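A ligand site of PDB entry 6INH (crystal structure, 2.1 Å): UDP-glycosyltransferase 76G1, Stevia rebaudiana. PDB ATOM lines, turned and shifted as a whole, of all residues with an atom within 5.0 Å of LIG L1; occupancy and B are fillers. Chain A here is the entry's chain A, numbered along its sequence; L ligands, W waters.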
ATOM      1  N   GLN A  23      11.346 -22.943  34.345  1.00  0.00           N
ATOM      2  CA  GLN A  23      11.900 -22.772  33.009  1.00  0.00           C
ATOM      3  C   GLN A  23      11.112 -21.796  32.123  1.00  0.00           C
ATOM      4  O   GLN A  23      11.696 -20.951  31.439  1.00  0.00           O
ATOM      5  CB  GLN A  23      11.993 -24.131  32.311  1.00  0.00           C
ATOM      6  CG  GLN A  23      12.797 -24.080  31.002  1.00  0.00           C
ATOM      7  CD  GLN A  23      14.291 -23.957  31.266  1.00  0.00           C
ATOM      8  OE1 GLN A  23      14.940 -24.960  31.511  1.00  0.00           O
ATOM      9  NE2 GLN A  23      14.816 -22.737  31.262  1.00  0.00           N
ATOM     10  N   GLY A  24       9.784 -21.912  32.166  1.00  0.00           N
ATOM     11  CA  GLY A  24       8.899 -21.093  31.343  1.00  0.00           C
ATOM     12  C   GLY A  24       8.769 -19.642  31.795  1.00  0.00           C
ATOM     13  O   GLY A  24       8.170 -18.831  31.112  1.00  0.00           O
ATOM     14  N   ASN A  27      13.076 -18.280  31.148  1.00  0.00           N
ATOM     15  CA  ASN A  27      13.383 -18.084  29.741  1.00  0.00           C
ATOM     16  C   ASN A  27      13.003 -16.679  29.222  1.00  0.00           C
ATOM     17  O   ASN A  27      13.894 -15.951  28.753  1.00  0.00           O
ATOM     18  CB  ASN A  27      12.792 -19.226  28.870  1.00  0.00           C
ATOM     19  CG  ASN A  27      13.590 -20.533  28.977  1.00  0.00           C
ATOM     20  OD1 ASN A  27      14.560 -20.599  29.720  1.00  0.00           O
ATOM     21  ND2 ASN A  27      13.188 -21.558  28.207  1.00  0.00           N
ATOM     22  N   ALA A 252      16.068 -19.002  23.896  1.00  0.00           N
ATOM     23  CA  ALA A 252      16.292 -19.139  25.336  1.00  0.00           C
ATOM     24  C   ALA A 252      17.319 -20.228  25.702  1.00  0.00           C
ATOM     25  O   ALA A 252      17.334 -20.698  26.852  1.00  0.00           O
ATOM     26  CB  ALA A 252      14.968 -19.430  26.034  1.00  0.00           C
ATOM     27  N   HIS A 260      21.575 -29.955  27.247  1.00  0.00           N
ATOM     28  CA  HIS A 260      21.018 -30.221  25.930  1.00  0.00           C
ATOM     29  C   HIS A 260      21.563 -31.516  25.334  1.00  0.00           C
ATOM     30  O   HIS A 260      22.745 -31.804  25.440  1.00  0.00           O
ATOM     31  CB  HIS A 260      21.350 -29.093  24.992  1.00  0.00           C
ATOM     32  CG  HIS A 260      20.672 -27.817  25.335  1.00  0.00           C
ATOM     33  ND1 HIS A 260      21.326 -26.605  25.332  1.00  0.00           N
ATOM     34  CD2 HIS A 260      19.389 -27.555  25.683  1.00  0.00           C
ATOM     35  CE1 HIS A 260      20.477 -25.647  25.667  1.00  0.00           C
ATOM     36  NE2 HIS A 260      19.298 -26.198  25.875  1.00  0.00           N
ATOM     37  N   TYR A 278       8.137 -33.017  16.013  1.00  0.00           N
ATOM     38  CA  TYR A 278       8.769 -32.737  17.297  1.00  0.00           C
ATOM     39  C   TYR A 278       7.690 -32.801  18.368  1.00  0.00           C
ATOM     40  O   TYR A 278       6.600 -32.232  18.198  1.00  0.00           O
ATOM     41  CB  TYR A 278       9.461 -31.368  17.288  1.00  0.00           C
ATOM     42  CG  TYR A 278      10.010 -30.923  18.626  1.00  0.00           C
ATOM     43  CD1 TYR A 278      11.119 -31.532  19.181  1.00  0.00           C
ATOM     44  CD2 TYR A 278       9.452 -29.837  19.299  1.00  0.00           C
ATOM     45  CE1 TYR A 278      11.612 -31.119  20.402  1.00  0.00           C
ATOM     46  CE2 TYR A 278       9.925 -29.420  20.507  1.00  0.00           C
ATOM     47  CZ  TYR A 278      11.021 -30.050  21.067  1.00  0.00           C
ATOM     48  OH  TYR A 278      11.523 -29.633  22.258  1.00  0.00           O
ATOM     49  N   SER A 280       7.098 -32.495  22.596  1.00  0.00           N
ATOM     50  CA  SER A 280       7.577 -32.154  23.932  1.00  0.00           C
ATOM     51  C   SER A 280       6.423 -31.589  24.725  1.00  0.00           C
ATOM     52  O   SER A 280       5.718 -30.695  24.232  1.00  0.00           O
ATOM     53  CB  SER A 280       8.687 -31.111  23.851  1.00  0.00           C
ATOM     54  OG  SER A 280       9.057 -30.702  25.165  1.00  0.00           O
ATOM     55  N   GLY A 282       6.916 -29.939  27.646  1.00  0.00           N
ATOM     56  CA  GLY A 282       7.436 -28.825  28.448  1.00  0.00           C
ATOM     57  C   GLY A 282       8.335 -29.236  29.596  1.00  0.00           C
ATOM     58  O   GLY A 282       8.967 -30.299  29.577  1.00  0.00           O
ATOM     59  N   SER A 283       8.364 -28.375  30.609  1.00  0.00           N
ATOM     60  CA  SER A 283       9.328 -28.499  31.716  1.00  0.00           C
ATOM     61  C   SER A 283       8.797 -29.058  33.041  1.00  0.00           C
ATOM     62  O   SER A 283       9.619 -29.470  33.866  1.00  0.00           O
ATOM     63  CB  SER A 283      10.032 -27.170  31.956  1.00  0.00           C
ATOM     64  OG  SER A 283       9.237 -26.254  32.671  1.00  0.00           O
ATOM     65  N   THR A 284       7.483 -29.063  33.249  1.00  0.00           N
ATOM     66  CA  THR A 284       6.901 -29.553  34.520  1.00  0.00           C
ATOM     67  C   THR A 284       5.807 -30.631  34.426  1.00  0.00           C
ATOM     68  O   THR A 284       5.440 -31.209  35.446  1.00  0.00           O
ATOM     69  CB  THR A 284       6.330 -28.380  35.355  1.00  0.00           C
ATOM     70  OG1 THR A 284       7.371 -27.424  35.630  1.00  0.00           O
ATOM     71  CG2 THR A 284       5.774 -28.886  36.659  1.00  0.00           C
ATOM     72  N   VAL A 309      10.987 -35.433  23.063  1.00  0.00           N
ATOM     73  CA  VAL A 309      11.621 -35.071  24.313  1.00  0.00           C
ATOM     74  C   VAL A 309      10.761 -35.590  25.445  1.00  0.00           C
ATOM     75  O   VAL A 309       9.619 -35.166  25.582  1.00  0.00           O
ATOM     76  CB  VAL A 309      11.796 -33.544  24.471  1.00  0.00           C
ATOM     77  CG1 VAL A 309      12.379 -33.218  25.828  1.00  0.00           C
ATOM     78  CG2 VAL A 309      12.696 -33.003  23.368  1.00  0.00           C
ATOM     79  N   LYS A 337      16.183 -36.538  26.345  1.00  0.00           N
ATOM     80  CA  LYS A 337      15.807 -35.928  27.617  1.00  0.00           C
ATOM     81  C   LYS A 337      15.509 -34.462  27.513  1.00  0.00           C
ATOM     82  O   LYS A 337      14.655 -33.951  28.254  1.00  0.00           O
ATOM     83  CB  LYS A 337      16.910 -36.152  28.652  1.00  0.00           C
ATOM     84  CG  LYS A 337      17.127 -37.615  28.988  1.00  0.00           C
ATOM     85  CD  LYS A 337      18.057 -37.761  30.178  1.00  0.00           C
ATOM     86  CE  LYS A 337      18.156 -39.199  30.672  1.00  0.00           C
ATOM     87  NZ  LYS A 337      19.105 -39.960  29.837  1.00  0.00           N
ATOM     88  N   TRP A 338      16.194 -33.770  26.603  1.00  0.00           N
ATOM     89  CA  TRP A 338      16.132 -32.315  26.562  1.00  0.00           C
ATOM     90  C   TRP A 338      16.900 -31.826  25.365  1.00  0.00           C
ATOM     91  O   TRP A 338      17.947 -32.369  25.065  1.00  0.00           O
ATOM     92  CB  TRP A 338      16.764 -31.747  27.825  1.00  0.00           C
ATOM     93  CG  TRP A 338      16.398 -30.322  28.081  1.00  0.00           C
ATOM     94  CD1 TRP A 338      17.206 -29.242  28.003  1.00  0.00           C
ATOM     95  CD2 TRP A 338      15.121 -29.843  28.495  1.00  0.00           C
ATOM     96  NE1 TRP A 338      16.528 -28.113  28.340  1.00  0.00           N
ATOM     97  CE2 TRP A 338      15.234 -28.444  28.643  1.00  0.00           C
ATOM     98  CE3 TRP A 338      13.895 -30.454  28.741  1.00  0.00           C
ATOM     99  CZ2 TRP A 338      14.159 -27.641  29.032  1.00  0.00           C
ATOM    100  CZ3 TRP A 338      12.827 -29.652  29.142  1.00  0.00           C
ATOM    101  CH2 TRP A 338      12.974 -28.261  29.278  1.00  0.00           C
ATOM    102  N   VAL A 339      16.390 -30.791  24.695  1.00  0.00           N
ATOM    103  CA  VAL A 339      17.029 -30.228  23.488  1.00  0.00           C
ATOM    104  C   VAL A 339      17.009 -28.698  23.560  1.00  0.00           C
ATOM    105  O   VAL A 339      16.344 -28.141  24.428  1.00  0.00           O
ATOM    106  CB  VAL A 339      16.287 -30.657  22.202  1.00  0.00           C
ATOM    107  CG1 VAL A 339      16.340 -32.166  22.048  1.00  0.00           C
ATOM    108  CG2 VAL A 339      14.841 -30.174  22.191  1.00  0.00           C
ATOM    109  N   PRO A 340      17.708 -28.009  22.650  1.00  0.00           N
ATOM    110  CA  PRO A 340      17.449 -26.569  22.498  1.00  0.00           C
ATOM    111  C   PRO A 340      16.224 -26.407  21.622  1.00  0.00           C
ATOM    112  O   PRO A 340      16.304 -26.475  20.399  1.00  0.00           O
ATOM    113  CB  PRO A 340      18.720 -26.038  21.821  1.00  0.00           C
ATOM    114  CG  PRO A 340      19.603 -27.219  21.591  1.00  0.00           C
ATOM    115  CD  PRO A 340      18.812 -28.465  21.799  1.00  0.00           C
ATOM    116  N   GLN A 341      15.077 -26.246  22.257  1.00  0.00           N
ATOM    117  CA  GLN A 341      13.803 -26.436  21.578  1.00  0.00           C
ATOM    118  C   GLN A 341      13.611 -25.483  20.405  1.00  0.00           C
ATOM    119  O   GLN A 341      13.233 -25.929  19.303  1.00  0.00           O
ATOM    120  CB  GLN A 341      12.633 -26.306  22.549  1.00  0.00           C
ATOM    121  CG  GLN A 341      11.304 -26.197  21.849  1.00  0.00           C
ATOM    122  CD  GLN A 341      10.143 -26.494  22.764  1.00  0.00           C
ATOM    123  OE1 GLN A 341      10.024 -27.612  23.282  1.00  0.00           O
ATOM    124  NE2 GLN A 341       9.287 -25.502  22.976  1.00  0.00           N
ATOM    125  N   GLN A 342      13.867 -24.195  20.599  1.00  0.00           N
ATOM    126  CA  GLN A 342      13.657 -23.262  19.466  1.00  0.00           C
ATOM    127  C   GLN A 342      14.566 -23.548  18.285  1.00  0.00           C
ATOM    128  O   GLN A 342      14.165 -23.425  17.115  1.00  0.00           O
ATOM    129  CB  GLN A 342      13.766 -21.800  19.891  1.00  0.00           C
ATOM    130  CG  GLN A 342      13.147 -20.890  18.831  1.00  0.00           C
ATOM    131  CD  GLN A 342      13.163 -19.427  19.218  1.00  0.00           C
ATOM    132  OE1 GLN A 342      13.279 -19.063  20.401  1.00  0.00           O
ATOM    133  NE2 GLN A 342      13.107 -18.582  18.201  1.00  0.00           N
ATOM    134  N   HIS A 356       2.310 -29.331  24.602  1.00  0.00           N
ATOM    135  CA  HIS A 356       1.382 -29.218  25.736  1.00  0.00           C
ATOM    136  C   HIS A 356       0.749 -27.836  25.813  1.00  0.00           C
ATOM    137  O   HIS A 356      -0.014 -27.583  26.737  1.00  0.00           O
ATOM    138  CB  HIS A 356       2.067 -29.537  27.070  1.00  0.00           C
ATOM    139  CG  HIS A 356       2.972 -28.457  27.572  1.00  0.00           C
ATOM    140  ND1 HIS A 356       3.975 -27.902  26.803  1.00  0.00           N
ATOM    141  CD2 HIS A 356       3.048 -27.861  28.792  1.00  0.00           C
ATOM    142  CE1 HIS A 356       4.601 -26.982  27.519  1.00  0.00           C
ATOM    143  NE2 HIS A 356       4.063 -26.934  28.721  1.00  0.00           N
ATOM    144  N   GLY A 358       2.060 -24.864  26.403  1.00  0.00           N
ATOM    145  CA  GLY A 358       2.697 -23.855  27.252  1.00  0.00           C
ATOM    146  C   GLY A 358       2.966 -22.643  26.374  1.00  0.00           C
ATOM    147  O   GLY A 358       3.207 -22.772  25.159  1.00  0.00           O
ATOM    148  N   TRP A 359       2.888 -21.465  26.940  1.00  0.00           N
ATOM    149  CA  TRP A 359       2.977 -20.287  26.111  1.00  0.00           C
ATOM    150  C   TRP A 359       4.310 -20.098  25.398  1.00  0.00           C
ATOM    151  O   TRP A 359       4.331 -19.736  24.233  1.00  0.00           O
ATOM    152  CB  TRP A 359       2.621 -19.051  26.897  1.00  0.00           C
ATOM    153  CG  TRP A 359       2.533 -17.856  26.030  1.00  0.00           C
ATOM    154  CD1 TRP A 359       3.332 -16.779  26.078  1.00  0.00           C
ATOM    155  CD2 TRP A 359       1.630 -17.644  24.938  1.00  0.00           C
ATOM    156  NE1 TRP A 359       2.970 -15.877  25.125  1.00  0.00           N
ATOM    157  CE2 TRP A 359       1.922 -16.379  24.402  1.00  0.00           C
ATOM    158  CE3 TRP A 359       0.597 -18.393  24.378  1.00  0.00           C
ATOM    159  CZ2 TRP A 359       1.228 -15.842  23.323  1.00  0.00           C
ATOM    160  CZ3 TRP A 359      -0.105 -17.861  23.303  1.00  0.00           C
ATOM    161  CH2 TRP A 359       0.209 -16.594  22.787  1.00  0.00           C
ATOM    162  N   ASN A 360       5.431 -20.349  26.079  1.00  0.00           N
ATOM    163  CA  ASN A 360       6.735 -20.194  25.419  1.00  0.00           C
ATOM    164  C   ASN A 360       6.855 -21.141  24.249  1.00  0.00           C
ATOM    165  O   ASN A 360       7.315 -20.747  23.200  1.00  0.00           O
ATOM    166  CB  ASN A 360       7.912 -20.411  26.389  1.00  0.00           C
ATOM    167  CG  ASN A 360       7.939 -19.376  27.477  1.00  0.00           C
ATOM    168  OD1 ASN A 360       8.376 -18.242  27.262  1.00  0.00           O
ATOM    169  ND2 ASN A 360       7.403 -19.748  28.644  1.00  0.00           N
ATOM    170  N   SER A 361       6.412 -22.381  24.441  1.00  0.00           N
ATOM    171  CA  SER A 361       6.488 -23.365  23.365  1.00  0.00           C
ATOM    172  C   SER A 361       5.612 -22.988  22.177  1.00  0.00           C
ATOM    173  O   SER A 361       6.026 -23.116  21.037  1.00  0.00           O
ATOM    174  CB  SER A 361       6.114 -24.755  23.878  1.00  0.00           C
ATOM    175  OG  SER A 361       7.106 -25.212  24.774  1.00  0.00           O
ATOM    176  N   GLU A 364       7.169 -19.902  20.476  1.00  0.00           N
ATOM    177  CA  GLU A 364       8.344 -20.359  19.739  1.00  0.00           C
ATOM    178  C   GLU A 364       7.965 -21.032  18.404  1.00  0.00           C
ATOM    179  O   GLU A 364       8.605 -20.785  17.386  1.00  0.00           O
ATOM    180  CB  GLU A 364       9.193 -21.318  20.568  1.00  0.00           C
ATOM    181  CG  GLU A 364       9.940 -20.651  21.720  1.00  0.00           C
ATOM    182  CD  GLU A 364      10.301 -21.584  22.882  1.00  0.00           C
ATOM    183  OE1 GLU A 364      10.285 -22.826  22.720  1.00  0.00           O
ATOM    184  OE2 GLU A 364      10.600 -21.070  23.970  1.00  0.00           O
ATOM    185  N   GLN A 381      -2.810 -23.559  29.476  1.00  0.00           N
ATOM    186  CA  GLN A 381      -2.612 -24.410  28.313  1.00  0.00           C
ATOM    187  C   GLN A 381      -3.861 -24.696  27.439  1.00  0.00           C
ATOM    188  O   GLN A 381      -3.777 -24.564  26.233  1.00  0.00           O
ATOM    189  CB  GLN A 381      -1.913 -25.698  28.705  1.00  0.00           C
ATOM    190  CG  GLN A 381      -0.501 -25.472  29.253  1.00  0.00           C
ATOM    191  CD  GLN A 381       0.000 -26.621  30.104  1.00  0.00           C
ATOM    192  OE1 GLN A 381      -0.472 -27.758  30.005  1.00  0.00           O
ATOM    193  NE2 GLN A 381       0.961 -26.330  30.952  1.00  0.00           N
HETATM  194  N1  LIG L   1      12.377 -26.285  26.365  1.00  0.00           N
HETATM  195  C1  LIG L   1      13.691 -26.577  25.949  1.00  0.00           C
HETATM  196  N2  LIG L   1      14.033 -27.833  25.650  1.00  0.00           N
HETATM  197  C2  LIG L   1      13.162 -28.836  25.731  1.00  0.00           C
HETATM  198  C3  LIG L   1      11.855 -28.581  26.123  1.00  0.00           C
HETATM  199  C4  LIG L   1      11.472 -27.275  26.442  1.00  0.00           C
HETATM  200  O1  LIG L   1      14.555 -25.685  25.861  1.00  0.00           O
HETATM  201  O2  LIG L   1      13.536 -30.004  25.438  1.00  0.00           O
HETATM  202  C5  LIG L   1      12.002 -24.904  26.704  1.00  0.00           C
HETATM  203  C6  LIG L   1      11.039 -24.302  25.675  1.00  0.00           C
HETATM  204  O3  LIG L   1      11.761 -23.826  24.544  1.00  0.00           O
HETATM  205  C7  LIG L   1      10.357 -23.218  26.466  1.00  0.00           C
HETATM  206  C8  LIG L   1      10.342 -23.791  27.891  1.00  0.00           C
HETATM  207  O4  LIG L   1      11.305 -24.854  27.938  1.00  0.00           O
HETATM  208  O5  LIG L   1      11.099 -21.996  26.406  1.00  0.00           O
HETATM  209  C9  LIG L   1       9.008 -24.396  28.271  1.00  0.00           C
HETATM  210  O6  LIG L   1       8.094 -23.332  28.514  1.00  0.00           O
HETATM  211  P1  LIG L   1       6.519 -23.498  28.291  1.00  0.00           P
HETATM  212  O7  LIG L   1       5.910 -22.170  28.626  1.00  0.00           O
HETATM  213  O8  LIG L   1       6.322 -24.019  26.886  1.00  0.00           O
HETATM  214  O9  LIG L   1       5.955 -24.667  29.241  1.00  0.00           O
HETATM  215  P2  LIG L   1       6.240 -24.997  30.799  1.00  0.00           P
HETATM  216  O10 LIG L   1       5.011 -25.801  31.108  1.00  0.00           O
HETATM  217  O11 LIG L   1       6.324 -23.656  31.486  1.00  0.00           O
HETATM  218  O12 LIG L   1       7.494 -25.796  30.789  1.00  0.00           O
HETATM  219  C1  LG2 L   2       1.473 -19.461  41.222  1.00  0.00           C
HETATM  220  C2  LG2 L   2       1.171 -21.654  40.060  1.00  0.00           C
HETATM  221  C3  LG2 L   2       0.907 -21.532  42.507  1.00  0.00           C
HETATM  222  C4  LG2 L   2      -1.093 -27.810  41.603  1.00  0.00           C
HETATM  223  C5  LG2 L   2      -0.992 -27.562  44.021  1.00  0.00           C
HETATM  224  C6  LG2 L   2       1.083 -23.915  43.061  1.00  0.00           C
HETATM  225  C7  LG2 L   2       0.643 -22.941  41.980  1.00  0.00           C
HETATM  226  C8  LG2 L   2       1.498 -22.994  40.713  1.00  0.00           C
HETATM  227  C9  LG2 L   2      -0.243 -21.638  39.513  1.00  0.00           C
HETATM  228  C10 LG2 L   2       2.524 -22.193  38.084  1.00  0.00           C
HETATM  229  O1  LG2 L   2       0.117 -27.974  41.307  1.00  0.00           O
HETATM  230  O2  LG2 L   2       4.900 -25.319  39.275  1.00  0.00           O
HETATM  231  C11 LG2 L   2       5.448 -24.447  38.280  1.00  0.00           C
HETATM  232  C12 LG2 L   2       4.307 -23.716  37.593  1.00  0.00           C
HETATM  233  C13 LG2 L   2       4.751 -22.868  36.394  1.00  0.00           C
HETATM  234  O3  LG2 L   2       5.477 -23.662  35.452  1.00  0.00           O
HETATM  235  C14 LG2 L   2       3.511 -22.270  35.740  1.00  0.00           C
HETATM  236  O4  LG2 L   2       3.873 -21.469  34.599  1.00  0.00           O
HETATM  237  O5  LG2 L   2       3.720 -22.838  38.554  1.00  0.00           O
HETATM  238  C15 LG2 L   2       2.765 -21.423  36.771  1.00  0.00           C
HETATM  239  O6  LG2 L   2       1.492 -21.029  36.255  1.00  0.00           O
HETATM  240  O7  LG2 L   2      -1.984 -28.430  40.968  1.00  0.00           O
HETATM  241  C16 LG2 L   2      -1.465 -26.861  42.744  1.00  0.00           C
HETATM  242  C17 LG2 L   2      -2.973 -26.716  42.872  1.00  0.00           C
HETATM  243  C18 LG2 L   2      -0.869 -25.433  42.631  1.00  0.00           C
HETATM  244  C19 LG2 L   2       0.670 -25.344  42.778  1.00  0.00           C
HETATM  245  C20 LG2 L   2       1.212 -20.763  41.248  1.00  0.00           C
HETATM  246  C21 LG2 L   2      -1.304 -22.083  40.545  1.00  0.00           C
HETATM  247  C22 LG2 L   2      -0.871 -23.091  41.651  1.00  0.00           C
HETATM  248  C23 LG2 L   2      -1.393 -24.555  41.458  1.00  0.00           C
HETATM  249  C24 LG2 L   2      -1.009 -25.128  40.071  1.00  0.00           C
HETATM  250  C25 LG2 L   2      -2.919 -24.538  41.493  1.00  0.00           C
HETATM  251  C26 LG2 L   2      -3.613 -25.873  41.776  1.00  0.00           C
HETATM  252  O8  LG2 L   2       2.118 -21.239  39.065  1.00  0.00           O
HETATM  253  O   HOH W   1      15.711 -23.094  27.746  1.00  0.00           O
HETATM  254  O   HOH W   2      13.860 -22.744  23.261  1.00  0.00           O
HETATM  255  O   HOH W   3       5.346 -28.513  31.491  1.00  0.00           O
HETATM  256  O   HOH W   4      16.968 -24.762  25.786  1.00  0.00           O
HETATM  257  O   HOH W   5       7.745 -23.261  33.755  1.00  0.00           O
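CG of Gln 23 touches O4 of LIG L1, 3.5 Å away.
Gly 24 touches LIG L1.
Tyr 278 touches LIG L1 (OH to O2, 3.8 Å).
Ser 280 touches LIG L1 (OG to C3, 3.6 Å).
Gly 282 touches LIG L1.
Val 309 touches LIG L1 (CG1 to O2, 3.4 Å).
CE2 of Trp 338 touches N2 of LIG L1, 3.3 Å away.
Gly 358 touches LIG L1 (CA to O8, 3.6 Å).
Trp 359 touches LIG L1.
Water W4 lies within hydrogen-bond range of O1 of LIG L1 and NE2 of His 260.
Water W2 lies within hydrogen-bond range of an oxygen (O3) of LIG L1 (2.7 Å) and the backbone NH of Gln 342 (3.0 Å).
Water W5 lies within hydrogen-bond range of O11 of LIG L1, O3 of LG2 L2 and N of Gly 24.
Water W3 lies within hydrogen-bond range of an oxygen (O10) of LIG L1 (2.8 Å), the backbone NH of Thr 284 (2.8 Å), the backbone NH of Ser 283 (3.1 Å) and a ring nitrogen (NE2) of His 356 (3.4 Å).
Water W1 lies within hydrogen-bond range of ND2 of Asn 27 (3.0 Å), O of Ala 252 (3.0 Å) and O1 of LIG L1 (3.4 Å).
OG of Ser 280 sits at hydrogen-bond distance from N of Gly 282, 3.4 Å away.
OG of Ser 361 lies within hydrogen-bond range of NE2 of Gln 341 (2.8 Å).
The side-chain amide oxygen (OD1) of Asn 27 sits at hydrogen-bond distance from the side-chain amide nitrogen (NE2) of Gln 23, 2.6 Å away.
The side-chain amide nitrogen (NE2) of Gln 341 sits at hydrogen-bond distance from the side-chain carboxylate (OE1) of Glu 364, 2.9 Å away.
O of His 356 lies close to OE1 of Gln 381 (3.3 Å).
The backbone carbonyl oxygen of Gly 24 lies within hydrogen-bond range of the side-chain amide nitrogen of Asn 360, at 2.7 Å.
The side-chain hydroxyl of Tyr 278 sits at hydrogen-bond distance from the side-chain amide oxygen of Gln 341 (2.7 Å).
O8 of LIG L1 is in hydrogen-bond range of N of Ser 361, at 2.9 Å.
The side-chain amide nitrogen (NE2) of Gln 341 sits close to an oxygen (O3) of LIG L1 (3.4 Å).
The backbone NH of Asn 360 lies within hydrogen-bond range of an oxygen (O7) of LIG L1 (3.2 Å).
The side-chain hydroxyl (OG) of Ser 283 is in hydrogen-bond range of an oxygen (O12) of LIG L1, 2.6 Å away.
The backbone NH of Ser 283 is in hydrogen-bond range of an oxygen (O12) of LIG L1 (2.7 Å).
N of Val 339 is in hydrogen-bond range of O2 of LIG L1, at 3.1 Å.
An oxygen (O10) of LIG L1 lies within hydrogen-bond range of a ring nitrogen (NE2) of His 356 (2.8 Å).
An oxygen (O5) of LIG L1 is in hydrogen-bond range of the side-chain amide nitrogen (ND2) of Asn 27 (2.8 Å).
The side-chain hydroxyl (OG) of Ser 361 is in hydrogen-bond range of an oxygen (O8) of LIG L1, 2.5 Å away.
O3 of LIG L1 sits at hydrogen-bond distance from OE1 of Glu 364 (2.6 Å).
The side-chain amide nitrogen of Asn 360 lies within hydrogen-bond range of an oxygen (O7) of LIG L1 (2.8 Å).
O of Val 339 is in hydrogen-bond range of N2 of LIG L1 (2.6 Å).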
